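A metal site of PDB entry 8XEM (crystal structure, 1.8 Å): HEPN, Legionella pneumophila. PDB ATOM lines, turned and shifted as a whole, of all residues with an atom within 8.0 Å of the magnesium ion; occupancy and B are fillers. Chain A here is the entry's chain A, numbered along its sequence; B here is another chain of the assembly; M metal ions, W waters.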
ATOM      1  N   GLN A  40     -13.964  -7.352  25.823  1.00  0.00           N
ATOM      2  CA  GLN A  40     -12.777  -7.493  24.985  1.00  0.00           C
ATOM      3  C   GLN A  40     -12.116  -8.854  25.186  1.00  0.00           C
ATOM      4  O   GLN A  40     -11.611  -9.465  24.235  1.00  0.00           O
ATOM      5  CB  GLN A  40     -11.775  -6.390  25.308  1.00  0.00           C
ATOM      6  CG  GLN A  40     -12.244  -4.969  25.049  1.00  0.00           C
ATOM      7  CD  GLN A  40     -12.620  -4.708  23.600  1.00  0.00           C
ATOM      8  OE1 GLN A  40     -12.052  -5.279  22.676  1.00  0.00           O
ATOM      9  NE2 GLN A  40     -13.555  -3.778  23.394  1.00  0.00           N
ATOM     10  N   GLY A  41     -12.116  -9.352  26.429  1.00  0.00           N
ATOM     11  CA  GLY A  41     -11.533 -10.667  26.681  1.00  0.00           C
ATOM     12  C   GLY A  41     -12.334 -11.795  26.049  1.00  0.00           C
ATOM     13  O   GLY A  41     -11.764 -12.784  25.560  1.00  0.00           O
ATOM     14  N   ILE A  43     -13.981 -11.527  23.322  1.00  0.00           N
ATOM     15  CA  ILE A  43     -13.616 -11.459  21.912  1.00  0.00           C
ATOM     16  C   ILE A  43     -12.279 -12.150  21.661  1.00  0.00           C
ATOM     17  O   ILE A  43     -12.142 -12.939  20.714  1.00  0.00           O
ATOM     18  CB  ILE A  43     -13.603  -9.986  21.449  1.00  0.00           C
ATOM     19  CG1 ILE A  43     -15.041  -9.456  21.414  1.00  0.00           C
ATOM     20  CG2 ILE A  43     -12.937  -9.853  20.099  1.00  0.00           C
ATOM     21  CD1 ILE A  43     -15.143  -7.952  21.337  1.00  0.00           C
ATOM     22  N   GLN A  44     -11.287 -11.879  22.509  1.00  0.00           N
ATOM     23  CA  GLN A  44      -9.987 -12.539  22.339  1.00  0.00           C
ATOM     24  C   GLN A  44     -10.106 -14.056  22.451  1.00  0.00           C
ATOM     25  O   GLN A  44      -9.462 -14.792  21.686  1.00  0.00           O
ATOM     26  CB  GLN A  44      -8.987 -12.010  23.371  1.00  0.00           C
ATOM     27  CG  GLN A  44      -7.603 -12.685  23.393  1.00  0.00           C
ATOM     28  CD  GLN A  44      -6.840 -12.606  22.075  1.00  0.00           C
ATOM     29  OE1 GLN A  44      -7.232 -11.901  21.155  1.00  0.00           O
ATOM     30  NE2 GLN A  44      -5.724 -13.325  22.011  1.00  0.00           N
ATOM     31  N   ALA A  45     -10.901 -14.552  23.406  1.00  0.00           N
ATOM     32  CA  ALA A  45     -11.073 -15.996  23.532  1.00  0.00           C
ATOM     33  C   ALA A  45     -11.770 -16.575  22.306  1.00  0.00           C
ATOM     34  O   ALA A  45     -11.425 -17.672  21.843  1.00  0.00           O
ATOM     35  CB  ALA A  45     -11.858 -16.336  24.798  1.00  0.00           C
ATOM     36  N   PHE A  46     -12.747 -15.850  21.758  1.00  0.00           N
ATOM     37  CA  PHE A  46     -13.344 -16.267  20.499  1.00  0.00           C
ATOM     38  C   PHE A  46     -12.281 -16.391  19.421  1.00  0.00           C
ATOM     39  O   PHE A  46     -12.261 -17.350  18.647  1.00  0.00           O
ATOM     40  CB  PHE A  46     -14.428 -15.284  20.050  1.00  0.00           C
ATOM     41  CG  PHE A  46     -14.647 -15.266  18.559  1.00  0.00           C
ATOM     42  CD1 PHE A  46     -15.175 -16.367  17.904  1.00  0.00           C
ATOM     43  CD2 PHE A  46     -14.328 -14.141  17.808  1.00  0.00           C
ATOM     44  CE1 PHE A  46     -15.377 -16.362  16.539  1.00  0.00           C
ATOM     45  CE2 PHE A  46     -14.517 -14.125  16.440  1.00  0.00           C
ATOM     46  CZ  PHE A  46     -15.042 -15.245  15.801  1.00  0.00           C
ATOM     47  N   GLU A  47     -11.381 -15.415  19.359  1.00  0.00           N
ATOM     48  CA  GLU A  47     -10.365 -15.416  18.308  1.00  0.00           C
ATOM     49  C   GLU A  47      -9.417 -16.595  18.456  1.00  0.00           C
ATOM     50  O   GLU A  47      -9.110 -17.271  17.456  1.00  0.00           O
ATOM     51  CB  GLU A  47      -9.619 -14.097  18.308  1.00  0.00           C
ATOM     52  CG  GLU A  47     -10.557 -12.958  17.930  1.00  0.00           C
ATOM     53  CD  GLU A  47      -9.890 -11.617  17.845  1.00  0.00           C
ATOM     54  OE1 GLU A  47      -8.732 -11.486  18.279  1.00  0.00           O
ATOM     55  OE2 GLU A  47     -10.549 -10.681  17.347  1.00  0.00           O
ATOM     56  N   PHE A  48      -8.936 -16.900  19.671  1.00  0.00           N
ATOM     57  CA  PHE A  48      -8.011 -18.031  19.740  1.00  0.00           C
ATOM     58  C   PHE A  48      -8.735 -19.367  19.603  1.00  0.00           C
ATOM     59  O   PHE A  48      -8.157 -20.331  19.059  1.00  0.00           O
ATOM     60  CB  PHE A  48      -7.072 -17.974  20.969  1.00  0.00           C
ATOM     61  CG  PHE A  48      -7.713 -18.028  22.361  1.00  0.00           C
ATOM     62  CD1 PHE A  48      -8.507 -19.079  22.769  1.00  0.00           C
ATOM     63  CD2 PHE A  48      -7.368 -17.059  23.308  1.00  0.00           C
ATOM     64  CE1 PHE A  48      -9.019 -19.123  24.072  1.00  0.00           C
ATOM     65  CE2 PHE A  48      -7.877 -17.099  24.602  1.00  0.00           C
ATOM     66  CZ  PHE A  48      -8.703 -18.136  24.982  1.00  0.00           C
ATOM     67  N   ARG A  98     -13.788 -12.165  12.848  1.00  0.00           N
ATOM     68  CA  ARG A  98     -12.348 -12.065  13.020  1.00  0.00           C
ATOM     69  C   ARG A  98     -11.806 -10.849  12.281  1.00  0.00           C
ATOM     70  O   ARG A  98     -10.902 -10.161  12.779  1.00  0.00           O
ATOM     71  CB  ARG A  98     -11.628 -13.313  12.503  1.00  0.00           C
ATOM     72  CG  ARG A  98     -11.935 -14.642  13.192  1.00  0.00           C
ATOM     73  CD  ARG A  98     -11.205 -14.857  14.517  1.00  0.00           C
ATOM     74  NE  ARG A  98      -9.777 -14.587  14.486  1.00  0.00           N
ATOM     75  CZ  ARG A  98      -8.834 -15.467  14.169  1.00  0.00           C
ATOM     76  NH1 ARG A  98      -9.129 -16.708  13.817  1.00  0.00           N
ATOM     77  NH2 ARG A  98      -7.553 -15.090  14.214  1.00  0.00           N
ATOM     78  N   THR A 101     -11.778  -7.426  14.185  1.00  0.00           N
ATOM     79  CA  THR A 101     -11.162  -7.402  15.508  1.00  0.00           C
ATOM     80  C   THR A 101     -10.525  -6.056  15.826  1.00  0.00           C
ATOM     81  O   THR A 101     -10.570  -5.584  16.973  1.00  0.00           O
ATOM     82  CB  THR A 101     -10.115  -8.510  15.606  1.00  0.00           C
ATOM     83  OG1 THR A 101      -9.591  -8.574  16.940  1.00  0.00           O
ATOM     84  CG2 THR A 101      -8.964  -8.279  14.632  1.00  0.00           C
ATOM     85  N   SER A 102      -9.934  -5.410  14.833  1.00  0.00           N
ATOM     86  CA  SER A 102      -9.221  -4.169  15.108  1.00  0.00           C
ATOM     87  C   SER A 102     -10.148  -3.014  15.470  1.00  0.00           C
ATOM     88  O   SER A 102      -9.650  -1.993  15.943  1.00  0.00           O
ATOM     89  CB  SER A 102      -8.369  -3.799  13.889  1.00  0.00           C
ATOM     90  OG  SER A 102      -9.176  -3.450  12.790  1.00  0.00           O
ATOM     91  N   THR A 104     -12.823  -3.127  17.718  1.00  0.00           N
ATOM     92  CA  THR A 104     -13.640  -3.327  18.920  1.00  0.00           C
ATOM     93  C   THR A 104     -13.418  -2.247  19.976  1.00  0.00           C
ATOM     94  O   THR A 104     -14.065  -2.290  21.029  1.00  0.00           O
ATOM     95  CB  THR A 104     -13.393  -4.717  19.529  1.00  0.00           C
ATOM     96  OG1 THR A 104     -12.066  -4.811  20.046  1.00  0.00           O
ATOM     97  CG2 THR A 104     -13.589  -5.807  18.489  1.00  0.00           C
ATOM     98  N   GLN B  40      -7.143 -11.382  28.993  1.00  0.00           N
ATOM     99  CA  GLN B  40      -7.455 -11.481  27.579  1.00  0.00           C
ATOM    100  C   GLN B  40      -7.959 -10.147  27.032  1.00  0.00           C
ATOM    101  O   GLN B  40      -7.629  -9.761  25.896  1.00  0.00           O
ATOM    102  CB  GLN B  40      -8.491 -12.589  27.345  1.00  0.00           C
ATOM    103  CG  GLN B  40      -8.105 -13.961  27.871  1.00  0.00           C
ATOM    104  CD  GLN B  40      -6.901 -14.543  27.155  1.00  0.00           C
ATOM    105  OE1 GLN B  40      -6.572 -14.125  26.044  1.00  0.00           O
ATOM    106  NE2 GLN B  40      -6.251 -15.525  27.780  1.00  0.00           N
ATOM    107  N   GLY B  41      -8.748  -9.425  27.822  1.00  0.00           N
ATOM    108  CA  GLY B  41      -9.250  -8.139  27.356  1.00  0.00           C
ATOM    109  C   GLY B  41      -8.162  -7.090  27.229  1.00  0.00           C
ATOM    110  O   GLY B  41      -8.156  -6.291  26.289  1.00  0.00           O
ATOM    111  N   ILE B  43      -5.110  -7.778  26.504  1.00  0.00           N
ATOM    112  CA  ILE B  43      -4.392  -8.152  25.294  1.00  0.00           C
ATOM    113  C   ILE B  43      -5.135  -7.636  24.060  1.00  0.00           C
ATOM    114  O   ILE B  43      -4.526  -7.078  23.138  1.00  0.00           O
ATOM    115  CB  ILE B  43      -4.173  -9.676  25.231  1.00  0.00           C
ATOM    116  CG1 ILE B  43      -3.187 -10.080  26.332  1.00  0.00           C
ATOM    117  CG2 ILE B  43      -3.666 -10.100  23.871  1.00  0.00           C
ATOM    118  CD1 ILE B  43      -3.179 -11.547  26.634  1.00  0.00           C
ATOM    119  N   GLN B  44      -6.456  -7.824  24.016  1.00  0.00           N
ATOM    120  CA  GLN B  44      -7.229  -7.322  22.891  1.00  0.00           C
ATOM    121  C   GLN B  44      -7.071  -5.804  22.747  1.00  0.00           C
ATOM    122  O   GLN B  44      -6.941  -5.281  21.626  1.00  0.00           O
ATOM    123  CB  GLN B  44      -8.703  -7.690  23.070  1.00  0.00           C
ATOM    124  CG  GLN B  44      -9.676  -7.170  22.001  1.00  0.00           C
ATOM    125  CD  GLN B  44      -9.343  -7.610  20.576  1.00  0.00           C
ATOM    126  OE1 GLN B  44      -8.615  -8.593  20.371  1.00  0.00           O
ATOM    127  NE2 GLN B  44      -9.900  -6.913  19.597  1.00  0.00           N
ATOM    128  N   ALA B  45      -7.099  -5.090  23.869  1.00  0.00           N
ATOM    129  CA  ALA B  45      -6.952  -3.632  23.809  1.00  0.00           C
ATOM    130  C   ALA B  45      -5.557  -3.256  23.333  1.00  0.00           C
ATOM    131  O   ALA B  45      -5.400  -2.284  22.576  1.00  0.00           O
ATOM    132  CB  ALA B  45      -7.242  -3.028  25.183  1.00  0.00           C
ATOM    133  N   PHE B  46      -4.532  -3.997  23.765  1.00  0.00           N
ATOM    134  CA  PHE B  46      -3.200  -3.817  23.195  1.00  0.00           C
ATOM    135  C   PHE B  46      -3.251  -3.998  21.685  1.00  0.00           C
ATOM    136  O   PHE B  46      -2.620  -3.235  20.939  1.00  0.00           O
ATOM    137  CB  PHE B  46      -2.218  -4.827  23.815  1.00  0.00           C
ATOM    138  CG  PHE B  46      -1.009  -5.105  22.959  1.00  0.00           C
ATOM    139  CD1 PHE B  46      -0.035  -4.141  22.768  1.00  0.00           C
ATOM    140  CD2 PHE B  46      -0.864  -6.342  22.323  1.00  0.00           C
ATOM    141  CE1 PHE B  46       1.079  -4.395  21.971  1.00  0.00           C
ATOM    142  CE2 PHE B  46       0.247  -6.609  21.530  1.00  0.00           C
ATOM    143  CZ  PHE B  46       1.209  -5.639  21.349  1.00  0.00           C
ATOM    144  N   GLU B  47      -3.977  -5.005  21.211  1.00  0.00           N
ATOM    145  CA  GLU B  47      -3.955  -5.297  19.792  1.00  0.00           C
ATOM    146  C   GLU B  47      -4.595  -4.176  18.980  1.00  0.00           C
ATOM    147  O   GLU B  47      -4.047  -3.755  17.955  1.00  0.00           O
ATOM    148  CB  GLU B  47      -4.628  -6.645  19.529  1.00  0.00           C
ATOM    149  CG  GLU B  47      -3.807  -7.776  20.123  1.00  0.00           C
ATOM    150  CD  GLU B  47      -4.400  -9.137  19.904  1.00  0.00           C
ATOM    151  OE1 GLU B  47      -5.583  -9.240  19.509  1.00  0.00           O
ATOM    152  OE2 GLU B  47      -3.671 -10.124  20.142  1.00  0.00           O
ATOM    153  N   PHE B  48      -5.732  -3.639  19.448  1.00  0.00           N
ATOM    154  CA  PHE B  48      -6.328  -2.572  18.628  1.00  0.00           C
ATOM    155  C   PHE B  48      -5.559  -1.258  18.783  1.00  0.00           C
ATOM    156  O   PHE B  48      -5.454  -0.482  17.809  1.00  0.00           O
ATOM    157  CB  PHE B  48      -7.858  -2.429  18.851  1.00  0.00           C
ATOM    158  CG  PHE B  48      -8.334  -2.068  20.251  1.00  0.00           C
ATOM    159  CD1 PHE B  48      -7.880  -0.939  20.927  1.00  0.00           C
ATOM    160  CD2 PHE B  48      -9.358  -2.808  20.829  1.00  0.00           C
ATOM    161  CE1 PHE B  48      -8.399  -0.619  22.180  1.00  0.00           C
ATOM    162  CE2 PHE B  48      -9.864  -2.486  22.077  1.00  0.00           C
ATOM    163  CZ  PHE B  48      -9.393  -1.388  22.745  1.00  0.00           C
ATOM    164  N   ARG B  98       2.013  -9.264  19.248  1.00  0.00           N
ATOM    165  CA  ARG B  98       0.912  -9.399  18.308  1.00  0.00           C
ATOM    166  C   ARG B  98       0.895 -10.810  17.735  1.00  0.00           C
ATOM    167  O   ARG B  98      -0.156 -11.457  17.628  1.00  0.00           O
ATOM    168  CB  ARG B  98       1.048  -8.387  17.173  1.00  0.00           C
ATOM    169  CG  ARG B  98       0.830  -6.915  17.522  1.00  0.00           C
ATOM    170  CD  ARG B  98      -0.609  -6.562  17.900  1.00  0.00           C
ATOM    171  NE  ARG B  98      -1.612  -6.948  16.895  1.00  0.00           N
ATOM    172  CZ  ARG B  98      -2.004  -6.200  15.879  1.00  0.00           C
ATOM    173  NH1 ARG B  98      -1.437  -5.028  15.620  1.00  0.00           N
ATOM    174  NH2 ARG B  98      -2.977  -6.632  15.093  1.00  0.00           N
ATOM    175  N   THR B 101      -0.747 -13.728  19.706  1.00  0.00           N
ATOM    176  CA  THR B 101      -2.154 -13.599  20.089  1.00  0.00           C
ATOM    177  C   THR B 101      -2.894 -14.933  20.095  1.00  0.00           C
ATOM    178  O   THR B 101      -3.728 -15.187  20.960  1.00  0.00           O
ATOM    179  CB  THR B 101      -2.847 -12.622  19.140  1.00  0.00           C
ATOM    180  OG1 THR B 101      -4.199 -12.415  19.564  1.00  0.00           O
ATOM    181  CG2 THR B 101      -2.855 -13.168  17.703  1.00  0.00           C
ATOM    182  N   SER B 102      -2.613 -15.789  19.111  1.00  0.00           N
ATOM    183  CA  SER B 102      -3.395 -17.009  18.993  1.00  0.00           C
ATOM    184  C   SER B 102      -3.080 -18.018  20.086  1.00  0.00           C
ATOM    185  O   SER B 102      -3.792 -19.022  20.210  1.00  0.00           O
ATOM    186  CB  SER B 102      -3.143 -17.637  17.630  1.00  0.00           C
ATOM    187  OG  SER B 102      -1.760 -17.894  17.457  1.00  0.00           O
ATOM    188  N   THR B 104      -2.749 -17.202  23.504  1.00  0.00           N
ATOM    189  CA  THR B 104      -2.988 -16.699  24.851  1.00  0.00           C
ATOM    190  C   THR B 104      -3.953 -17.564  25.646  1.00  0.00           C
ATOM    191  O   THR B 104      -4.254 -17.231  26.796  1.00  0.00           O
ATOM    192  CB  THR B 104      -3.511 -15.249  24.825  1.00  0.00           C
ATOM    193  OG1 THR B 104      -4.816 -15.207  24.224  1.00  0.00           O
ATOM    194  CG2 THR B 104      -2.549 -14.356  24.064  1.00  0.00           C
HETATM  195 MG    MG M   1      -7.438 -10.411  19.520  1.00  0.00          MG
HETATM  196  O   HOH W   1      -6.201 -13.464  18.405  1.00  0.00           O
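Merely in contact with the magnesium ion: Thr 101 of chain B (3.8 Å) and Thr 101 of chain A (3.8 Å).
Of the 24 residues printed, 6 come within 4 Å of the magnesium ion.
Along chain A the residues within 4 Å of the magnesium ion span positions 44 to 101.
The magnesium ion is bound by OE1 of Glu 47 of chain A (2.1 Å), OE1 of Glu 47 of chain B (2.2 Å), OE1 of Gln 44 of chain A (2.2 Å) and OE1 of Gln 44 of chain B (2.3 Å).
The magnesium ion has four donor atoms within binding distance.
The side-chain carboxylate (OE1) of Glu 47 of chain A sits close to the side-chain hydroxyl (OG1) of Thr 101 of chain A.
The side-chain hydroxyl (OG1) of Thr 101 of chain B is in hydrogen-bond range of the side-chain carboxylate (OE2) of Glu 47 of chain B (2.4 Å).
The side-chain amide nitrogen of Gln 44 of chain A lies within hydrogen-bond range of the backbone carbonyl oxygen of Thr 101 of chain B, at 2.9 Å.
The side-chain amide nitrogen (NE2) of Gln 44 of chain A sits at hydrogen-bond distance from the side-chain hydroxyl (OG1) of Thr 104 of chain B (3.0 Å).
NE2 of Gln 44 of chain B sits at hydrogen-bond distance from O of Thr 101 of chain A (3.0 Å).
The side-chain amide nitrogen of Gln 44 of chain B is in hydrogen-bond range of the side-chain hydroxyl of Thr 104 of chain A (3.1 Å).
OG1 of Thr 104 of chain B sits close to O of Thr 101 of chain B, 3.4 Å away.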
